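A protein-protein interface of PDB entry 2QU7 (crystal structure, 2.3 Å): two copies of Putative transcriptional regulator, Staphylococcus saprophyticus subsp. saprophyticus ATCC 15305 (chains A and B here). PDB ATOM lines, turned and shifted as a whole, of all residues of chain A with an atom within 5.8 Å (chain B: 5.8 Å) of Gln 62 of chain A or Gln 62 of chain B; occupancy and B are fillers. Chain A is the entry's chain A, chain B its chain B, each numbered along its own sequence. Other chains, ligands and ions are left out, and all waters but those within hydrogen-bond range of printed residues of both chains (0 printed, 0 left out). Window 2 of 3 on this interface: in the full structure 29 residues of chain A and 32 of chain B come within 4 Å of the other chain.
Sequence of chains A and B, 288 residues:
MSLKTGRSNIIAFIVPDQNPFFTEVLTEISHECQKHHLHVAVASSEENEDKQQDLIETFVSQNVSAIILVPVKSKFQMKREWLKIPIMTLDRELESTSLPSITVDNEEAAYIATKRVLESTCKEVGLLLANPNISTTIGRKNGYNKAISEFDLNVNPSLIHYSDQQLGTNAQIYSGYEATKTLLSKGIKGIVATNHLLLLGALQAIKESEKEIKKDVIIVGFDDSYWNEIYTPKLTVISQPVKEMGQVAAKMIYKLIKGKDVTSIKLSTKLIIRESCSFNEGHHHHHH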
ATOM      1  N   ARG A   7       0.688   9.586 -29.964  1.00  0.00           N
ATOM      2  CA  ARG A   7       0.353   8.324 -29.226  1.00  0.00           C
ATOM      3  C   ARG A   7       1.650   7.569 -28.881  1.00  0.00           C
ATOM      4  O   ARG A   7       2.342   7.075 -29.771  1.00  0.00           O
ATOM      5  CB  ARG A   7      -0.612   7.483 -30.068  1.00  0.00           C
ATOM      6  CG  ARG A   7      -1.378   6.352 -29.379  1.00  0.00           C
ATOM      7  CD  ARG A   7      -2.494   6.786 -28.366  1.00  0.00           C
ATOM      8  NE  ARG A   7      -3.619   7.622 -28.825  1.00  0.00           N
ATOM      9  CZ  ARG A   7      -4.884   7.203 -28.996  1.00  0.00           C
ATOM     10  NH1 ARG A   7      -5.218   5.929 -28.812  1.00  0.00           N
ATOM     11  NH2 ARG A   7      -5.830   8.060 -29.376  1.00  0.00           N
ATOM     12  N   SER A   8       1.993   7.517 -27.594  1.00  0.00           N
ATOM     13  CA  SER A   8       3.253   6.919 -27.148  1.00  0.00           C
ATOM     14  C   SER A   8       3.180   5.393 -27.099  1.00  0.00           C
ATOM     15  O   SER A   8       2.092   4.822 -27.010  1.00  0.00           O
ATOM     16  CB  SER A   8       3.645   7.467 -25.781  1.00  0.00           C
ATOM     17  OG  SER A   8       2.758   6.958 -24.801  1.00  0.00           O
ATOM     18  N   ILE A  10       3.623   3.382 -24.813  1.00  0.00           N
ATOM     19  CA  ILE A  10       3.394   2.924 -23.447  1.00  0.00           C
ATOM     20  C   ILE A  10       1.976   2.401 -23.229  1.00  0.00           C
ATOM     21  O   ILE A  10       1.004   2.979 -23.727  1.00  0.00           O
ATOM     22  CB  ILE A  10       3.803   4.011 -22.424  1.00  0.00           C
ATOM     23  CG1 ILE A  10       5.311   3.892 -22.148  1.00  0.00           C
ATOM     24  CG2 ILE A  10       3.033   3.861 -21.092  1.00  0.00           C
ATOM     25  CD1 ILE A  10       5.966   5.195 -21.850  1.00  0.00           C
ATOM     26  N   GLU A  57      -6.565  10.117 -15.859  1.00  0.00           N
ATOM     27  CA  GLU A  57      -6.445  11.460 -16.449  1.00  0.00           C
ATOM     28  C   GLU A  57      -5.014  11.763 -16.922  1.00  0.00           C
ATOM     29  O   GLU A  57      -4.792  12.416 -17.948  1.00  0.00           O
ATOM     30  CB  GLU A  57      -6.918  12.546 -15.452  1.00  0.00           C
ATOM     31  CG  GLU A  57      -8.279  13.192 -15.779  1.00  0.00           C
ATOM     32  CD  GLU A  57      -9.079  13.642 -14.522  1.00  0.00           C
ATOM     33  OE1 GLU A  57      -8.479  14.217 -13.573  1.00  0.00           O
ATOM     34  OE2 GLU A  57     -10.312  13.411 -14.494  1.00  0.00           O
ATOM     35  N   THR A  58      -4.048  11.303 -16.142  1.00  0.00           N
ATOM     36  CA  THR A  58      -2.648  11.518 -16.450  1.00  0.00           C
ATOM     37  C   THR A  58      -2.223  10.722 -17.688  1.00  0.00           C
ATOM     38  O   THR A  58      -1.505  11.242 -18.551  1.00  0.00           O
ATOM     39  CB  THR A  58      -1.776  11.177 -15.231  1.00  0.00           C
ATOM     40  OG1 THR A  58      -2.051  12.141 -14.199  1.00  0.00           O
ATOM     41  CG2 THR A  58      -0.275  11.206 -15.596  1.00  0.00           C
ATOM     42  N   PHE A  59      -2.670   9.475 -17.784  1.00  0.00           N
ATOM     43  CA  PHE A  59      -2.249   8.643 -18.899  1.00  0.00           C
ATOM     44  C   PHE A  59      -2.983   9.021 -20.186  1.00  0.00           C
ATOM     45  O   PHE A  59      -2.399   8.949 -21.270  1.00  0.00           O
ATOM     46  CB  PHE A  59      -2.359   7.153 -18.565  1.00  0.00           C
ATOM     47  CG  PHE A  59      -1.357   6.701 -17.538  1.00  0.00           C
ATOM     48  CD1 PHE A  59       0.012   6.923 -17.729  1.00  0.00           C
ATOM     49  CD2 PHE A  59      -1.770   6.067 -16.378  1.00  0.00           C
ATOM     50  CE1 PHE A  59       0.958   6.522 -16.769  1.00  0.00           C
ATOM     51  CE2 PHE A  59      -0.833   5.647 -15.410  1.00  0.00           C
ATOM     52  CZ  PHE A  59       0.528   5.876 -15.605  1.00  0.00           C
ATOM     53  N   VAL A  60      -4.232   9.472 -20.047  1.00  0.00           N
ATOM     54  CA  VAL A  60      -4.988  10.000 -21.178  1.00  0.00           C
ATOM     55  C   VAL A  60      -4.280  11.240 -21.756  1.00  0.00           C
ATOM     56  O   VAL A  60      -4.098  11.347 -22.971  1.00  0.00           O
ATOM     57  CB  VAL A  60      -6.490  10.288 -20.828  1.00  0.00           C
ATOM     58  CG1 VAL A  60      -7.212  10.926 -22.002  1.00  0.00           C
ATOM     59  CG2 VAL A  60      -7.207   8.999 -20.445  1.00  0.00           C
ATOM     60  N   SER A  61      -3.861  12.143 -20.877  1.00  0.00           N
ATOM     61  CA  SER A  61      -3.193  13.386 -21.268  1.00  0.00           C
ATOM     62  C   SER A  61      -1.866  13.113 -21.950  1.00  0.00           C
ATOM     63  O   SER A  61      -1.420  13.885 -22.787  1.00  0.00           O
ATOM     64  CB  SER A  61      -2.964  14.292 -20.047  1.00  0.00           C
ATOM     65  OG  SER A  61      -4.217  14.658 -19.482  1.00  0.00           O
ATOM     66  N   GLN A  62      -1.232  12.009 -21.589  1.00  0.00           N
ATOM     67  CA  GLN A  62       0.052  11.674 -22.191  1.00  0.00           C
ATOM     68  C   GLN A  62      -0.092  10.818 -23.445  1.00  0.00           C
ATOM     69  O   GLN A  62       0.895  10.441 -24.076  1.00  0.00           O
ATOM     70  CB  GLN A  62       0.980  11.060 -21.146  1.00  0.00           C
ATOM     71  CG  GLN A  62       1.634  12.142 -20.262  1.00  0.00           C
ATOM     72  CD  GLN A  62       2.415  13.201 -21.100  1.00  0.00           C
ATOM     73  OE1 GLN A  62       2.013  14.378 -21.178  1.00  0.00           O
ATOM     74  NE2 GLN A  62       3.526  12.771 -21.735  1.00  0.00           N
ATOM     75  N   ASN A  63      -1.333  10.528 -23.817  1.00  0.00           N
ATOM     76  CA  ASN A  63      -1.604   9.830 -25.065  1.00  0.00           C
ATOM     77  C   ASN A  63      -0.964   8.450 -25.167  1.00  0.00           C
ATOM     78  O   ASN A  63      -0.392   8.097 -26.219  1.00  0.00           O
ATOM     79  CB  ASN A  63      -1.190  10.689 -26.263  1.00  0.00           C
ATOM     80  CG  ASN A  63      -2.365  11.359 -26.915  1.00  0.00           C
ATOM     81  OD1 ASN A  63      -3.086  10.740 -27.725  1.00  0.00           O
ATOM     82  ND2 ASN A  63      -2.589  12.627 -26.563  1.00  0.00           N
ATOM     83  N   VAL A  64      -1.096   7.681 -24.079  1.00  0.00           N
ATOM     84  CA  VAL A  64      -0.642   6.300 -24.020  1.00  0.00           C
ATOM     85  C   VAL A  64      -1.408   5.495 -25.073  1.00  0.00           C
ATOM     86  O   VAL A  64      -2.487   5.917 -25.500  1.00  0.00           O
ATOM     87  CB  VAL A  64      -0.799   5.692 -22.575  1.00  0.00           C
ATOM     88  CG1 VAL A  64       0.073   6.439 -21.546  1.00  0.00           C
ATOM     89  CG2 VAL A  64      -2.281   5.632 -22.115  1.00  0.00           C
ATOM     90  N   ARG B   7       5.622  19.764 -19.457  1.00  0.00           N
ATOM     91  CA  ARG B   7       6.078  18.436 -18.946  1.00  0.00           C
ATOM     92  C   ARG B   7       4.899  17.577 -18.498  1.00  0.00           C
ATOM     93  O   ARG B   7       3.887  18.080 -18.011  1.00  0.00           O
ATOM     94  CB  ARG B   7       7.082  18.585 -17.801  1.00  0.00           C
ATOM     95  CG  ARG B   7       8.479  19.024 -18.236  1.00  0.00           C
ATOM     96  CD  ARG B   7       9.423  17.864 -18.545  1.00  0.00           C
ATOM     97  NE  ARG B   7      10.532  18.236 -19.431  1.00  0.00           N
ATOM     98  CZ  ARG B   7      11.689  18.793 -19.046  1.00  0.00           C
ATOM     99  NH1 ARG B   7      11.928  19.085 -17.767  1.00  0.00           N
ATOM    100  NH2 ARG B   7      12.626  19.073 -19.955  1.00  0.00           N
ATOM    101  N   SER B   8       5.042  16.276 -18.693  1.00  0.00           N
ATOM    102  CA  SER B   8       4.126  15.279 -18.139  1.00  0.00           C
ATOM    103  C   SER B   8       4.337  15.245 -16.631  1.00  0.00           C
ATOM    104  O   SER B   8       5.462  15.431 -16.171  1.00  0.00           O
ATOM    105  CB  SER B   8       4.457  13.928 -18.762  1.00  0.00           C
ATOM    106  OG  SER B   8       4.124  12.860 -17.916  1.00  0.00           O
ATOM    107  N   ASN B   9       3.273  15.030 -15.855  1.00  0.00           N
ATOM    108  CA  ASN B   9       3.420  14.949 -14.391  1.00  0.00           C
ATOM    109  C   ASN B   9       3.792  13.540 -13.877  1.00  0.00           C
ATOM    110  O   ASN B   9       3.484  13.146 -12.749  1.00  0.00           O
ATOM    111  CB  ASN B   9       2.205  15.546 -13.664  1.00  0.00           C
ATOM    112  CG  ASN B   9       0.927  14.774 -13.913  1.00  0.00           C
ATOM    113  OD1 ASN B   9       0.822  14.021 -14.877  1.00  0.00           O
ATOM    114  ND2 ASN B   9      -0.067  14.979 -13.056  1.00  0.00           N
ATOM    115  N   ILE B  10       4.456  12.778 -14.730  1.00  0.00           N
ATOM    116  CA  ILE B  10       4.858  11.431 -14.393  1.00  0.00           C
ATOM    117  C   ILE B  10       6.318  11.434 -14.035  1.00  0.00           C
ATOM    118  O   ILE B  10       7.115  12.051 -14.733  1.00  0.00           O
ATOM    119  CB  ILE B  10       4.698  10.504 -15.599  1.00  0.00           C
ATOM    120  CG1 ILE B  10       3.234  10.316 -15.923  1.00  0.00           C
ATOM    121  CG2 ILE B  10       5.367   9.136 -15.350  1.00  0.00           C
ATOM    122  CD1 ILE B  10       3.018   9.696 -17.282  1.00  0.00           C
ATOM    123  N   GLU B  57      14.398   5.961 -23.517  1.00  0.00           N
ATOM    124  CA  GLU B  57      14.100   6.637 -24.766  1.00  0.00           C
ATOM    125  C   GLU B  57      12.623   7.000 -24.881  1.00  0.00           C
ATOM    126  O   GLU B  57      12.302   8.081 -25.346  1.00  0.00           O
ATOM    127  CB  GLU B  57      14.547   5.754 -25.936  1.00  0.00           C
ATOM    128  CG  GLU B  57      14.020   6.154 -27.295  1.00  0.00           C
ATOM    129  CD  GLU B  57      14.584   5.253 -28.399  1.00  0.00           C
ATOM    130  OE1 GLU B  57      13.995   4.160 -28.631  1.00  0.00           O
ATOM    131  OE2 GLU B  57      15.622   5.635 -29.009  1.00  0.00           O
ATOM    132  N   THR B  58      11.734   6.096 -24.461  1.00  0.00           N
ATOM    133  CA  THR B  58      10.299   6.398 -24.439  1.00  0.00           C
ATOM    134  C   THR B  58       9.955   7.485 -23.421  1.00  0.00           C
ATOM    135  O   THR B  58       9.160   8.367 -23.711  1.00  0.00           O
ATOM    136  CB  THR B  58       9.422   5.186 -24.111  1.00  0.00           C
ATOM    137  OG1 THR B  58       9.724   4.105 -25.002  1.00  0.00           O
ATOM    138  CG2 THR B  58       7.992   5.567 -24.334  1.00  0.00           C
ATOM    139  N   PHE B  59      10.551   7.418 -22.232  1.00  0.00           N
ATOM    140  CA  PHE B  59      10.247   8.398 -21.212  1.00  0.00           C
ATOM    141  C   PHE B  59      10.777   9.787 -21.545  1.00  0.00           C
ATOM    142  O   PHE B  59      10.076  10.772 -21.289  1.00  0.00           O
ATOM    143  CB  PHE B  59      10.663   7.915 -19.818  1.00  0.00           C
ATOM    144  CG  PHE B  59       9.841   6.765 -19.320  1.00  0.00           C
ATOM    145  CD1 PHE B  59       8.440   6.847 -19.302  1.00  0.00           C
ATOM    146  CD2 PHE B  59      10.451   5.603 -18.876  1.00  0.00           C
ATOM    147  CE1 PHE B  59       7.658   5.776 -18.844  1.00  0.00           C
ATOM    148  CE2 PHE B  59       9.687   4.512 -18.411  1.00  0.00           C
ATOM    149  CZ  PHE B  59       8.287   4.598 -18.394  1.00  0.00           C
ATOM    150  N   VAL B  60      11.976   9.854 -22.138  1.00  0.00           N
ATOM    151  CA  VAL B  60      12.517  11.109 -22.686  1.00  0.00           C
ATOM    152  C   VAL B  60      11.575  11.687 -23.730  1.00  0.00           C
ATOM    153  O   VAL B  60      11.242  12.871 -23.678  1.00  0.00           O
ATOM    154  CB  VAL B  60      13.913  10.937 -23.328  1.00  0.00           C
ATOM    155  CG1 VAL B  60      14.358  12.229 -24.017  1.00  0.00           C
ATOM    156  CG2 VAL B  60      14.960  10.498 -22.289  1.00  0.00           C
ATOM    157  N   SER B  61      11.126  10.837 -24.661  1.00  0.00           N
ATOM    158  CA  SER B  61      10.223  11.260 -25.734  1.00  0.00           C
ATOM    159  C   SER B  61       8.884  11.784 -25.189  1.00  0.00           C
ATOM    160  O   SER B  61       8.308  12.751 -25.713  1.00  0.00           O
ATOM    161  CB  SER B  61       9.966  10.103 -26.685  1.00  0.00           C
ATOM    162  OG  SER B  61       9.291  10.569 -27.829  1.00  0.00           O
ATOM    163  N   GLN B  62       8.409  11.147 -24.125  1.00  0.00           N
ATOM    164  CA  GLN B  62       7.175  11.550 -23.478  1.00  0.00           C
ATOM    165  C   GLN B  62       7.355  12.816 -22.640  1.00  0.00           C
ATOM    166  O   GLN B  62       6.380  13.365 -22.146  1.00  0.00           O
ATOM    167  CB  GLN B  62       6.676  10.445 -22.562  1.00  0.00           C
ATOM    168  CG  GLN B  62       5.915   9.350 -23.224  1.00  0.00           C
ATOM    169  CD  GLN B  62       5.073   8.589 -22.211  1.00  0.00           C
ATOM    170  OE1 GLN B  62       3.872   8.274 -22.442  1.00  0.00           O
ATOM    171  NE2 GLN B  62       5.679   8.316 -21.060  1.00  0.00           N
ATOM    172  N   ASN B  63       8.592  13.277 -22.478  1.00  0.00           N
ATOM    173  CA  ASN B  63       8.857  14.427 -21.617  1.00  0.00           C
ATOM    174  C   ASN B  63       8.390  14.317 -20.156  1.00  0.00           C
ATOM    175  O   ASN B  63       7.847  15.285 -19.590  1.00  0.00           O
ATOM    176  CB  ASN B  63       8.260  15.690 -22.209  1.00  0.00           C
ATOM    177  CG  ASN B  63       9.302  16.674 -22.547  1.00  0.00           C
ATOM    178  OD1 ASN B  63       9.515  17.648 -21.799  1.00  0.00           O
ATOM    179  ND2 ASN B  63      10.035  16.413 -23.652  1.00  0.00           N
ATOM    180  N   VAL B  64       8.595  13.153 -19.547  1.00  0.00           N
ATOM    181  CA  VAL B  64       8.256  12.987 -18.133  1.00  0.00           C
ATOM    182  C   VAL B  64       8.961  14.070 -17.305  1.00  0.00           C
ATOM    183  O   VAL B  64       9.979  14.626 -17.739  1.00  0.00           O
ATOM    184  CB  VAL B  64       8.589  11.555 -17.643  1.00  0.00           C
ATOM    185  CG1 VAL B  64       7.865  10.516 -18.511  1.00  0.00           C
ATOM    186  CG2 VAL B  64      10.099  11.302 -17.665  1.00  0.00           C
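The side-chain hydroxyl of Thr 58 of chain A lies close to the side-chain amide oxygen of Asn 9 of chain B (3.5 Å).
The side-chain amide nitrogen of Gln 62 of chain A sits at hydrogen-bond distance from the backbone carbonyl oxygen of Gln 62 of chain B (2.9 Å).
OG of Ser 8 of chain A lies within hydrogen-bond range of OE1 of Gln 62 of chain B (2.9 Å).
N of Ser 8 of chain A lies within hydrogen-bond range of O of Asn 63 of chain A (2.8 Å).
The backbone carbonyl oxygen of Phe 59 of chain B is in hydrogen-bond range of the backbone NH of Val 64 of chain B (3.3 Å).
OG of Ser 8 of chain B sits close to N of Ile 10 of chain B, at 3.2 Å.
The backbone carbonyl oxygen (O) of Phe 59 of chain A lies within hydrogen-bond range of the backbone NH (N) of Val 64 of chain A, 3.3 Å away.
N of Ser 8 of chain B is in hydrogen-bond range of O of Asn 63 of chain B (3.1 Å).
Among the printed residues, pairs that only touch across the chains: Gln 62 of chain A with Ser 8 of chain B, Ile 10 of chain A with Thr 58 of chain B, Ile 10 of chain A with Gln 62 of chain B, Ile 10 of chain A with Phe 59 of chain B, Thr 58 of chain A with Ile 10 of chain B and Phe 59 of chain A with Ile 10 of chain B.
Of chain B, only Ser 8 (3.2 Å) and Gln 62 (2.9 Å) come within 4 Å of Gln 62 of chain A.
Of the printed residues of chain A, Asn 9 of chain B touches Thr 58.
Of the printed residues of chain A, Phe 59 of chain B touches Ile 10 (3.5 Å).
Ser 61 of chain B touches none of the printed residues of chain A.
Of chain A, only Ser 8, Ile 10 and Gln 62 come within 4 Å of Gln 62 of chain B.
The nearest residue of chain B that does not touch Gln 62 of chain A is Ile 10 of chain B (4.1 Å).
The nearest printed residue of chain A that does not touch Phe 59 of chain B is Gln 62 of chain A (6.9 Å).
Printed residues of chain A that touch a printed residue of chain B: Ser 8, Ile 10, Thr 58, Phe 59 and Gln 62.
Hydrophobic or aromatic side chains of chain A that line the printed part of chain B: Ile 10 and Phe 59.
Of the 12 printed residues of chain B, 6 touch a printed residue of chain A.
Hydrophobic or aromatic side chains of chain B within 4 Å of the printed part of chain A: Ile 10 and Phe 59.
Among the printed residues, 9 pairs touch across the chains.
Ser 8 of chain A touches Gln 62 of chain B, and with the chains exchanged Gln 62 of chain A touches Ser 8 of chain B.
Ile 10 of chain A touches Phe 59 of chain B, and with the chains exchanged Phe 59 of chain A touches Ile 10 of chain B.
Ile 10 of chain A touches Gln 62 of chain B, but with the chains exchanged Gln 62 of chain A does not touch Ile 10 of chain B (4.1 Å).
Gln 62 of chain A touches its own counterpart, Gln 62 of chain B.
Positions printed for both chains: 7, 8, 10, 57, 58, 59, 60, 61, 62, 63 and 64.
Of the 9 pairs that touch across the chains among the printed residues, 7 have their exchanged pair printed and touching as well.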
